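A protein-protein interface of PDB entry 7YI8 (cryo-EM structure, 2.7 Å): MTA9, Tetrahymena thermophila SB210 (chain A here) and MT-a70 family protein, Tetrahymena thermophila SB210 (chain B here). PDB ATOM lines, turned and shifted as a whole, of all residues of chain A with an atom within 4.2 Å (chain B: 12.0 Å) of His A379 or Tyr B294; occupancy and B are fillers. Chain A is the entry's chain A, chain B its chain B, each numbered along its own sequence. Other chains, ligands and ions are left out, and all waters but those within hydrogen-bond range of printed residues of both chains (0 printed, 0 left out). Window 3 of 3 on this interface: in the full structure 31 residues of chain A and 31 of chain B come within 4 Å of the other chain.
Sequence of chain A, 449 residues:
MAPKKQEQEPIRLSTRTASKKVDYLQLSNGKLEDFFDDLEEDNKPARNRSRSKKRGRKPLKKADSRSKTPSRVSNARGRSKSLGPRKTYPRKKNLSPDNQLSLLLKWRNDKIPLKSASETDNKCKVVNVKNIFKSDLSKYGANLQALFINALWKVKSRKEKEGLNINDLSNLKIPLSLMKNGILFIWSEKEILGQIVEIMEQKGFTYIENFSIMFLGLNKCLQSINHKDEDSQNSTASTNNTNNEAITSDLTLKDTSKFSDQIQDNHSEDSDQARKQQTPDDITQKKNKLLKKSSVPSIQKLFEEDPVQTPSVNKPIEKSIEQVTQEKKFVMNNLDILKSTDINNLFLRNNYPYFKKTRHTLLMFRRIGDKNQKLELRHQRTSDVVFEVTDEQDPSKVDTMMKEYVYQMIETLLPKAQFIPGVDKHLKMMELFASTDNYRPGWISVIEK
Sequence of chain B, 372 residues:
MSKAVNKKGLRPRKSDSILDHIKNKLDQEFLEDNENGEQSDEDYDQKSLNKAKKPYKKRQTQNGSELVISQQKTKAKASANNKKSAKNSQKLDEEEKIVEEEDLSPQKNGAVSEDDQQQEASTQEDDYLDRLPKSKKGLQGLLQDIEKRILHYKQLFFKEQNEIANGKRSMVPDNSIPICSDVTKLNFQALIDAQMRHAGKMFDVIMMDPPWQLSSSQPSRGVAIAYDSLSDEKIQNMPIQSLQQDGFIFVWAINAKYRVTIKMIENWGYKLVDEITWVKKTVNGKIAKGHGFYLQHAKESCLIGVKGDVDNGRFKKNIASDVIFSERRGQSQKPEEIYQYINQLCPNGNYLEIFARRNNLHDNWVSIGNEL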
ATOM      1  N   ILE A 208      -3.480  25.212 -13.850  1.00  0.00           N
ATOM      2  CA  ILE A 208      -3.684  24.193 -14.871  1.00  0.00           C
ATOM      3  C   ILE A 208      -2.568  23.153 -14.867  1.00  0.00           C
ATOM      4  O   ILE A 208      -2.834  21.949 -14.911  1.00  0.00           O
ATOM      5  CB  ILE A 208      -3.846  24.816 -16.276  1.00  0.00           C
ATOM      6  CG1 ILE A 208      -2.769  25.867 -16.542  1.00  0.00           C
ATOM      7  CG2 ILE A 208      -5.238  25.400 -16.435  1.00  0.00           C
ATOM      8  CD1 ILE A 208      -2.573  26.200 -17.998  1.00  0.00           C
ATOM      9  N   GLU A 209      -1.311  23.594 -14.825  1.00  0.00           N
ATOM     10  CA  GLU A 209      -0.230  22.653 -15.091  1.00  0.00           C
ATOM     11  C   GLU A 209       0.956  22.876 -14.167  1.00  0.00           C
ATOM     12  O   GLU A 209       1.091  23.909 -13.508  1.00  0.00           O
ATOM     13  CB  GLU A 209       0.242  22.736 -16.550  1.00  0.00           C
ATOM     14  CG  GLU A 209      -0.530  21.847 -17.509  1.00  0.00           C
ATOM     15  CD  GLU A 209      -0.153  20.382 -17.392  1.00  0.00           C
ATOM     16  OE1 GLU A 209       0.784  20.063 -16.632  1.00  0.00           O
ATOM     17  OE2 GLU A 209      -0.793  19.547 -18.064  1.00  0.00           O
ATOM     18  N   ARG A 366      -3.714  29.574 -15.682  1.00  0.00           N
ATOM     19  CA  ARG A 366      -4.447  29.979 -16.872  1.00  0.00           C
ATOM     20  C   ARG A 366      -5.496  31.025 -16.516  1.00  0.00           C
ATOM     21  O   ARG A 366      -6.068  31.009 -15.423  1.00  0.00           O
ATOM     22  CB  ARG A 366      -5.118  28.775 -17.540  1.00  0.00           C
ATOM     23  CG  ARG A 366      -5.833  29.087 -18.838  1.00  0.00           C
ATOM     24  CD  ARG A 366      -4.897  28.982 -20.020  1.00  0.00           C
ATOM     25  NE  ARG A 366      -5.597  28.560 -21.225  1.00  0.00           N
ATOM     26  CZ  ARG A 366      -6.271  29.376 -22.024  1.00  0.00           C
ATOM     27  NH1 ARG A 366      -6.356  30.671 -21.773  1.00  0.00           N
ATOM     28  NH2 ARG A 366      -6.874  28.878 -23.100  1.00  0.00           N
ATOM     29  N   LEU A 377      -3.028  26.405 -29.022  1.00  0.00           N
ATOM     30  CA  LEU A 377      -1.838  25.750 -28.506  1.00  0.00           C
ATOM     31  C   LEU A 377      -1.521  24.493 -29.312  1.00  0.00           C
ATOM     32  O   LEU A 377      -2.325  24.019 -30.119  1.00  0.00           O
ATOM     33  CB  LEU A 377      -2.003  25.383 -27.029  1.00  0.00           C
ATOM     34  CG  LEU A 377      -1.859  26.488 -25.980  1.00  0.00           C
ATOM     35  CD1 LEU A 377      -3.043  27.433 -26.003  1.00  0.00           C
ATOM     36  CD2 LEU A 377      -1.662  25.902 -24.592  1.00  0.00           C
ATOM     37  N   ARG A 378      -0.326  23.954 -29.077  1.00  0.00           N
ATOM     38  CA  ARG A 378       0.127  22.737 -29.735  1.00  0.00           C
ATOM     39  C   ARG A 378       0.143  21.536 -28.793  1.00  0.00           C
ATOM     40  O   ARG A 378       0.493  20.429 -29.219  1.00  0.00           O
ATOM     41  CB  ARG A 378       1.513  22.969 -30.354  1.00  0.00           C
ATOM     42  CG  ARG A 378       1.970  21.920 -31.363  1.00  0.00           C
ATOM     43  CD  ARG A 378       0.968  21.735 -32.493  1.00  0.00           C
ATOM     44  NE  ARG A 378       0.025  20.658 -32.210  1.00  0.00           N
ATOM     45  CZ  ARG A 378      -1.045  20.386 -32.942  1.00  0.00           C
ATOM     46  NH1 ARG A 378      -1.345  21.093 -34.019  1.00  0.00           N
ATOM     47  NH2 ARG A 378      -1.835  19.377 -32.586  1.00  0.00           N
ATOM     48  N   HIS A 379      -0.229  21.730 -27.525  1.00  0.00           N
ATOM     49  CA  HIS A 379      -0.476  20.647 -26.573  1.00  0.00           C
ATOM     50  C   HIS A 379       0.782  19.857 -26.228  1.00  0.00           C
ATOM     51  O   HIS A 379       1.828  20.440 -25.924  1.00  0.00           O
ATOM     52  CB  HIS A 379      -1.560  19.705 -27.107  1.00  0.00           C
ATOM     53  CG  HIS A 379      -2.737  20.415 -27.698  1.00  0.00           C
ATOM     54  ND1 HIS A 379      -3.671  21.077 -26.930  1.00  0.00           N
ATOM     55  CD2 HIS A 379      -3.130  20.572 -28.985  1.00  0.00           C
ATOM     56  CE1 HIS A 379      -4.588  21.608 -27.717  1.00  0.00           C
ATOM     57  NE2 HIS A 379      -4.283  21.317 -28.969  1.00  0.00           N
ATOM     58  N   GLN A 380       0.685  18.527 -26.271  1.00  0.00           N
ATOM     59  CA  GLN A 380       1.716  17.642 -25.727  1.00  0.00           C
ATOM     60  C   GLN A 380       2.878  17.540 -26.711  1.00  0.00           C
ATOM     61  O   GLN A 380       3.003  16.594 -27.492  1.00  0.00           O
ATOM     62  CB  GLN A 380       1.138  16.264 -25.418  1.00  0.00           C
ATOM     63  CG  GLN A 380       0.218  16.204 -24.204  1.00  0.00           C
ATOM     64  CD  GLN A 380      -1.101  16.918 -24.426  1.00  0.00           C
ATOM     65  OE1 GLN A 380      -1.433  17.869 -23.719  1.00  0.00           O
ATOM     66  NE2 GLN A 380      -1.866  16.455 -25.407  1.00  0.00           N
ATOM     67  N   ARG A 381       3.752  18.546 -26.665  1.00  0.00           N
ATOM     68  CA  ARG A 381       4.991  18.534 -27.428  1.00  0.00           C
ATOM     69  C   ARG A 381       6.234  18.461 -26.555  1.00  0.00           C
ATOM     70  O   ARG A 381       7.319  18.177 -27.075  1.00  0.00           O
ATOM     71  CB  ARG A 381       5.076  19.775 -28.328  1.00  0.00           C
ATOM     72  CG  ARG A 381       4.008  19.844 -29.410  1.00  0.00           C
ATOM     73  CD  ARG A 381       4.157  18.728 -30.440  1.00  0.00           C
ATOM     74  NE  ARG A 381       3.492  17.492 -30.043  1.00  0.00           N
ATOM     75  CZ  ARG A 381       3.678  16.320 -30.635  1.00  0.00           C
ATOM     76  NH1 ARG A 381       4.500  16.187 -31.662  1.00  0.00           N
ATOM     77  NH2 ARG A 381       3.023  15.253 -30.182  1.00  0.00           N
ATOM     78  N   ILE B 254      -4.648  13.928  -8.367  1.00  0.00           N
ATOM     79  CA  ILE B 254      -4.497  13.980  -9.815  1.00  0.00           C
ATOM     80  C   ILE B 254      -4.439  15.445 -10.230  1.00  0.00           C
ATOM     81  O   ILE B 254      -4.731  16.337  -9.427  1.00  0.00           O
ATOM     82  CB  ILE B 254      -5.638  13.237 -10.531  1.00  0.00           C
ATOM     83  CG1 ILE B 254      -6.994  13.812 -10.122  1.00  0.00           C
ATOM     84  CG2 ILE B 254      -5.579  11.754 -10.216  1.00  0.00           C
ATOM     85  CD1 ILE B 254      -8.162  13.210 -10.871  1.00  0.00           C
ATOM     86  N   ASN B 255      -4.054  15.703 -11.481  1.00  0.00           N
ATOM     87  CA  ASN B 255      -3.913  17.083 -11.934  1.00  0.00           C
ATOM     88  C   ASN B 255      -5.241  17.825 -11.871  1.00  0.00           C
ATOM     89  O   ASN B 255      -5.290  18.994 -11.468  1.00  0.00           O
ATOM     90  CB  ASN B 255      -3.348  17.119 -13.353  1.00  0.00           C
ATOM     91  CG  ASN B 255      -2.580  18.392 -13.639  1.00  0.00           C
ATOM     92  OD1 ASN B 255      -1.981  18.983 -12.741  1.00  0.00           O
ATOM     93  ND2 ASN B 255      -2.602  18.828 -14.890  1.00  0.00           N
ATOM     94  N   ALA B 256      -6.331  17.162 -12.260  1.00  0.00           N
ATOM     95  CA  ALA B 256      -7.640  17.804 -12.265  1.00  0.00           C
ATOM     96  C   ALA B 256      -8.134  18.145 -10.865  1.00  0.00           C
ATOM     97  O   ALA B 256      -9.041  18.972 -10.729  1.00  0.00           O
ATOM     98  CB  ALA B 256      -8.659  16.910 -12.969  1.00  0.00           C
ATOM     99  N   LYS B 289       5.173   7.511 -20.812  1.00  0.00           N
ATOM    100  CA  LYS B 289       4.402   8.618 -21.359  1.00  0.00           C
ATOM    101  C   LYS B 289       2.915   8.333 -21.219  1.00  0.00           C
ATOM    102  O   LYS B 289       2.443   7.263 -21.617  1.00  0.00           O
ATOM    103  CB  LYS B 289       4.753   8.858 -22.831  1.00  0.00           C
ATOM    104  CG  LYS B 289       6.216   9.209 -23.112  1.00  0.00           C
ATOM    105  CD  LYS B 289       6.594  10.606 -22.627  1.00  0.00           C
ATOM    106  CE  LYS B 289       7.194  10.589 -21.227  1.00  0.00           C
ATOM    107  NZ  LYS B 289       7.658  11.933 -20.801  1.00  0.00           N
ATOM    108  N   GLY B 290       2.180   9.292 -20.655  1.00  0.00           N
ATOM    109  CA  GLY B 290       0.745   9.203 -20.527  1.00  0.00           C
ATOM    110  C   GLY B 290       0.049  10.338 -21.259  1.00  0.00           C
ATOM    111  O   GLY B 290       0.683  11.193 -21.884  1.00  0.00           O
ATOM    112  N   HIS B 291      -1.279  10.323 -21.174  1.00  0.00           N
ATOM    113  CA  HIS B 291      -2.068  11.390 -21.768  1.00  0.00           C
ATOM    114  C   HIS B 291      -1.840  12.691 -21.011  1.00  0.00           C
ATOM    115  O   HIS B 291      -1.703  12.699 -19.786  1.00  0.00           O
ATOM    116  CB  HIS B 291      -3.554  11.030 -21.762  1.00  0.00           C
ATOM    117  CG  HIS B 291      -4.430  12.078 -22.375  1.00  0.00           C
ATOM    118  ND1 HIS B 291      -4.928  13.145 -21.660  1.00  0.00           N
ATOM    119  CD2 HIS B 291      -4.894  12.223 -23.639  1.00  0.00           C
ATOM    120  CE1 HIS B 291      -5.661  13.902 -22.455  1.00  0.00           C
ATOM    121  NE2 HIS B 291      -5.658  13.366 -23.662  1.00  0.00           N
ATOM    122  N   GLY B 292      -1.803  13.794 -21.747  1.00  0.00           N
ATOM    123  CA  GLY B 292      -1.502  15.083 -21.160  1.00  0.00           C
ATOM    124  C   GLY B 292      -2.583  16.103 -21.443  1.00  0.00           C
ATOM    125  O   GLY B 292      -3.306  16.020 -22.435  1.00  0.00           O
ATOM    126  N   PHE B 293      -2.681  17.080 -20.540  1.00  0.00           N
ATOM    127  CA  PHE B 293      -3.644  18.162 -20.709  1.00  0.00           C
ATOM    128  C   PHE B 293      -3.017  19.334 -21.454  1.00  0.00           C
ATOM    129  O   PHE B 293      -3.620  19.888 -22.379  1.00  0.00           O
ATOM    130  CB  PHE B 293      -4.175  18.597 -19.341  1.00  0.00           C
ATOM    131  CG  PHE B 293      -5.366  19.508 -19.410  1.00  0.00           C
ATOM    132  CD1 PHE B 293      -6.602  19.021 -19.803  1.00  0.00           C
ATOM    133  CD2 PHE B 293      -5.260  20.841 -19.059  1.00  0.00           C
ATOM    134  CE1 PHE B 293      -7.704  19.853 -19.862  1.00  0.00           C
ATOM    135  CE2 PHE B 293      -6.359  21.677 -19.113  1.00  0.00           C
ATOM    136  CZ  PHE B 293      -7.581  21.182 -19.515  1.00  0.00           C
ATOM    137  N   TYR B 294      -1.803  19.723 -21.063  1.00  0.00           N
ATOM    138  CA  TYR B 294      -1.030  20.710 -21.807  1.00  0.00           C
ATOM    139  C   TYR B 294       0.371  20.167 -22.057  1.00  0.00           C
ATOM    140  O   TYR B 294       1.008  20.504 -23.062  1.00  0.00           O
ATOM    141  CB  TYR B 294      -0.971  22.036 -21.048  1.00  0.00           C
ATOM    142  CG  TYR B 294      -2.220  22.874 -21.188  1.00  0.00           C
ATOM    143  CD1 TYR B 294      -2.953  23.253 -20.072  1.00  0.00           C
ATOM    144  CD2 TYR B 294      -2.671  23.281 -22.435  1.00  0.00           C
ATOM    145  CE1 TYR B 294      -4.097  24.016 -20.194  1.00  0.00           C
ATOM    146  CE2 TYR B 294      -3.813  24.045 -22.567  1.00  0.00           C
ATOM    147  CZ  TYR B 294      -4.522  24.411 -21.444  1.00  0.00           C
ATOM    148  OH  TYR B 294      -5.660  25.171 -21.570  1.00  0.00           O
ATOM    149  N   LEU B 295       0.854  19.326 -21.146  1.00  0.00           N
ATOM    150  CA  LEU B 295       2.127  18.638 -21.285  1.00  0.00           C
ATOM    151  C   LEU B 295       1.913  17.147 -21.069  1.00  0.00           C
ATOM    152  O   LEU B 295       1.007  16.739 -20.340  1.00  0.00           O
ATOM    153  CB  LEU B 295       3.165  19.162 -20.285  1.00  0.00           C
ATOM    154  CG  LEU B 295       3.581  20.628 -20.409  1.00  0.00           C
ATOM    155  CD1 LEU B 295       4.416  21.042 -19.212  1.00  0.00           C
ATOM    156  CD2 LEU B 295       4.340  20.861 -21.703  1.00  0.00           C
ATOM    157  N   GLN B 296       2.759  16.336 -21.705  1.00  0.00           N
ATOM    158  CA  GLN B 296       2.664  14.886 -21.567  1.00  0.00           C
ATOM    159  C   GLN B 296       2.874  14.466 -20.120  1.00  0.00           C
ATOM    160  O   GLN B 296       3.991  14.546 -19.603  1.00  0.00           O
ATOM    161  CB  GLN B 296       3.690  14.191 -22.464  1.00  0.00           C
ATOM    162  CG  GLN B 296       3.137  13.694 -23.783  1.00  0.00           C
ATOM    163  CD  GLN B 296       4.206  13.585 -24.849  1.00  0.00           C
ATOM    164  OE1 GLN B 296       5.398  13.677 -24.559  1.00  0.00           O
ATOM    165  NE2 GLN B 296       3.785  13.385 -26.092  1.00  0.00           N
ATOM    166  N   HIS B 297       1.813  13.998 -19.467  1.00  0.00           N
ATOM    167  CA  HIS B 297       1.885  13.656 -18.051  1.00  0.00           C
ATOM    168  C   HIS B 297       2.755  12.423 -17.848  1.00  0.00           C
ATOM    169  O   HIS B 297       2.433  11.338 -18.342  1.00  0.00           O
ATOM    170  CB  HIS B 297       0.483  13.421 -17.495  1.00  0.00           C
ATOM    171  CG  HIS B 297      -0.213  14.674 -17.064  1.00  0.00           C
ATOM    172  ND1 HIS B 297      -0.903  15.481 -17.942  1.00  0.00           N
ATOM    173  CD2 HIS B 297      -0.324  15.258 -15.848  1.00  0.00           C
ATOM    174  CE1 HIS B 297      -1.410  16.509 -17.285  1.00  0.00           C
ATOM    175  NE2 HIS B 297      -1.073  16.398 -16.013  1.00  0.00           N
ATOM    176  N   ALA B 298       3.857  12.591 -17.114  1.00  0.00           N
ATOM    177  CA  ALA B 298       4.778  11.497 -16.835  1.00  0.00           C
ATOM    178  C   ALA B 298       5.059  11.355 -15.344  1.00  0.00           C
ATOM    179  O   ALA B 298       6.069  10.759 -14.963  1.00  0.00           O
ATOM    180  CB  ALA B 298       6.090  11.684 -17.602  1.00  0.00           C
ATOM    181  N   LYS B 299       4.187  11.890 -14.494  1.00  0.00           N
ATOM    182  CA  LYS B 299       4.399  11.838 -13.056  1.00  0.00           C
ATOM    183  C   LYS B 299       3.065  12.037 -12.356  1.00  0.00           C
ATOM    184  O   LYS B 299       2.077  12.449 -12.968  1.00  0.00           O
ATOM    185  CB  LYS B 299       5.414  12.891 -12.602  1.00  0.00           C
ATOM    186  CG  LYS B 299       4.875  14.310 -12.600  1.00  0.00           C
ATOM    187  CD  LYS B 299       6.005  15.323 -12.597  1.00  0.00           C
ATOM    188  CE  LYS B 299       5.535  16.672 -12.088  1.00  0.00           C
ATOM    189  NZ  LYS B 299       4.473  17.240 -12.960  1.00  0.00           N
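The side-chain amide oxygen (OE1) of Gln A380 sits close to the backbone carbonyl oxygen (O) of Gly B292 (2.9 Å).
The backbone carbonyl oxygen of Tyr B294 lies close to the backbone carbonyl oxygen of His A379 (3.0 Å).
OE2 of Glu A209 sits at hydrogen-bond distance from N of Tyr B294 (3.2 Å).
NE of Arg A366 lies within hydrogen-bond range of OH of Tyr B294, 3.4 Å away.
The backbone NH (N) of Tyr B294 is in hydrogen-bond range of the side-chain amide oxygen (OE1) of Gln A380, 3.3 Å away.
O of Phe B293 sits close to OE1 of Gln A380, 3.3 Å away.
ND2 of Asn B255 lies within hydrogen-bond range of O of Ile A208 (3.1 Å).
The backbone carbonyl oxygen (O) of His B291 sits close to a ring nitrogen (ND1) of His B297 (3.4 Å).
The side-chain amide nitrogen of Asn B255 is in hydrogen-bond range of a ring nitrogen (NE2) of His B297 (3.1 Å).
A ring nitrogen (ND1) of His B297 sits at hydrogen-bond distance from the backbone carbonyl oxygen (O) of Leu B295 (3.3 Å).
The backbone NH (N) of Gly B290 is in hydrogen-bond range of the backbone carbonyl oxygen (O) of His B297.
Ile A208 touches Tyr B294.
Asn B255 touches Glu A209.
Phe B293 touches Glu A209 (CB to OE2, 3.7 Å).
Leu B295 touches Glu A209 (N to OE2, 3.5 Å).
CE1 of His B297 touches OE2 of Glu A209, 3.2 Å away.
Leu A377 touches Tyr B294 (CD2 to CE2, 3.5 Å).
CG of Gln A380 touches C of Leu B295, at 3.7 Å.
Gln B296 touches Gln A380 (N to CG, 3.6 Å).
Of chain B, only Tyr B294 comes within 4 Å of His A379.
Ile A208 touches just these residues of chain B: Asn B255 and Tyr B294.
Of chain B, only Asn B255 (3.7 Å), Phe B293 (3.7 Å), Tyr B294 (3.2 Å), Leu B295 (3.5 Å) and His B297 (3.2 Å) come within 4 Å of Glu A209.
Leu A377 touches one residue of chain B.
No residue of chain B comes within 4 Å of Arg A378.
Of chain B, only Gly B292 (2.9 Å), Phe B293 (3.1 Å), Tyr B294 (3.3 Å), Leu B295 (3.7 Å) and Gln B296 (3.6 Å) come within 4 Å of Gln A380.
No residue of chain B comes within 4 Å of Arg A381.
Printed residues of chain A within 4 Å of Gln B296: Gln A380 (3.6 Å).
Of the printed residues of chain B, Arg A366 touches Tyr B294.
Ala B256 touches none of the printed residues of chain A.
The nearest printed residue of chain A that does not touch Tyr B294 is Arg A381 (4.9 Å).
Of the 14 printed residues of chain B, 7 touch a printed residue of chain A.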
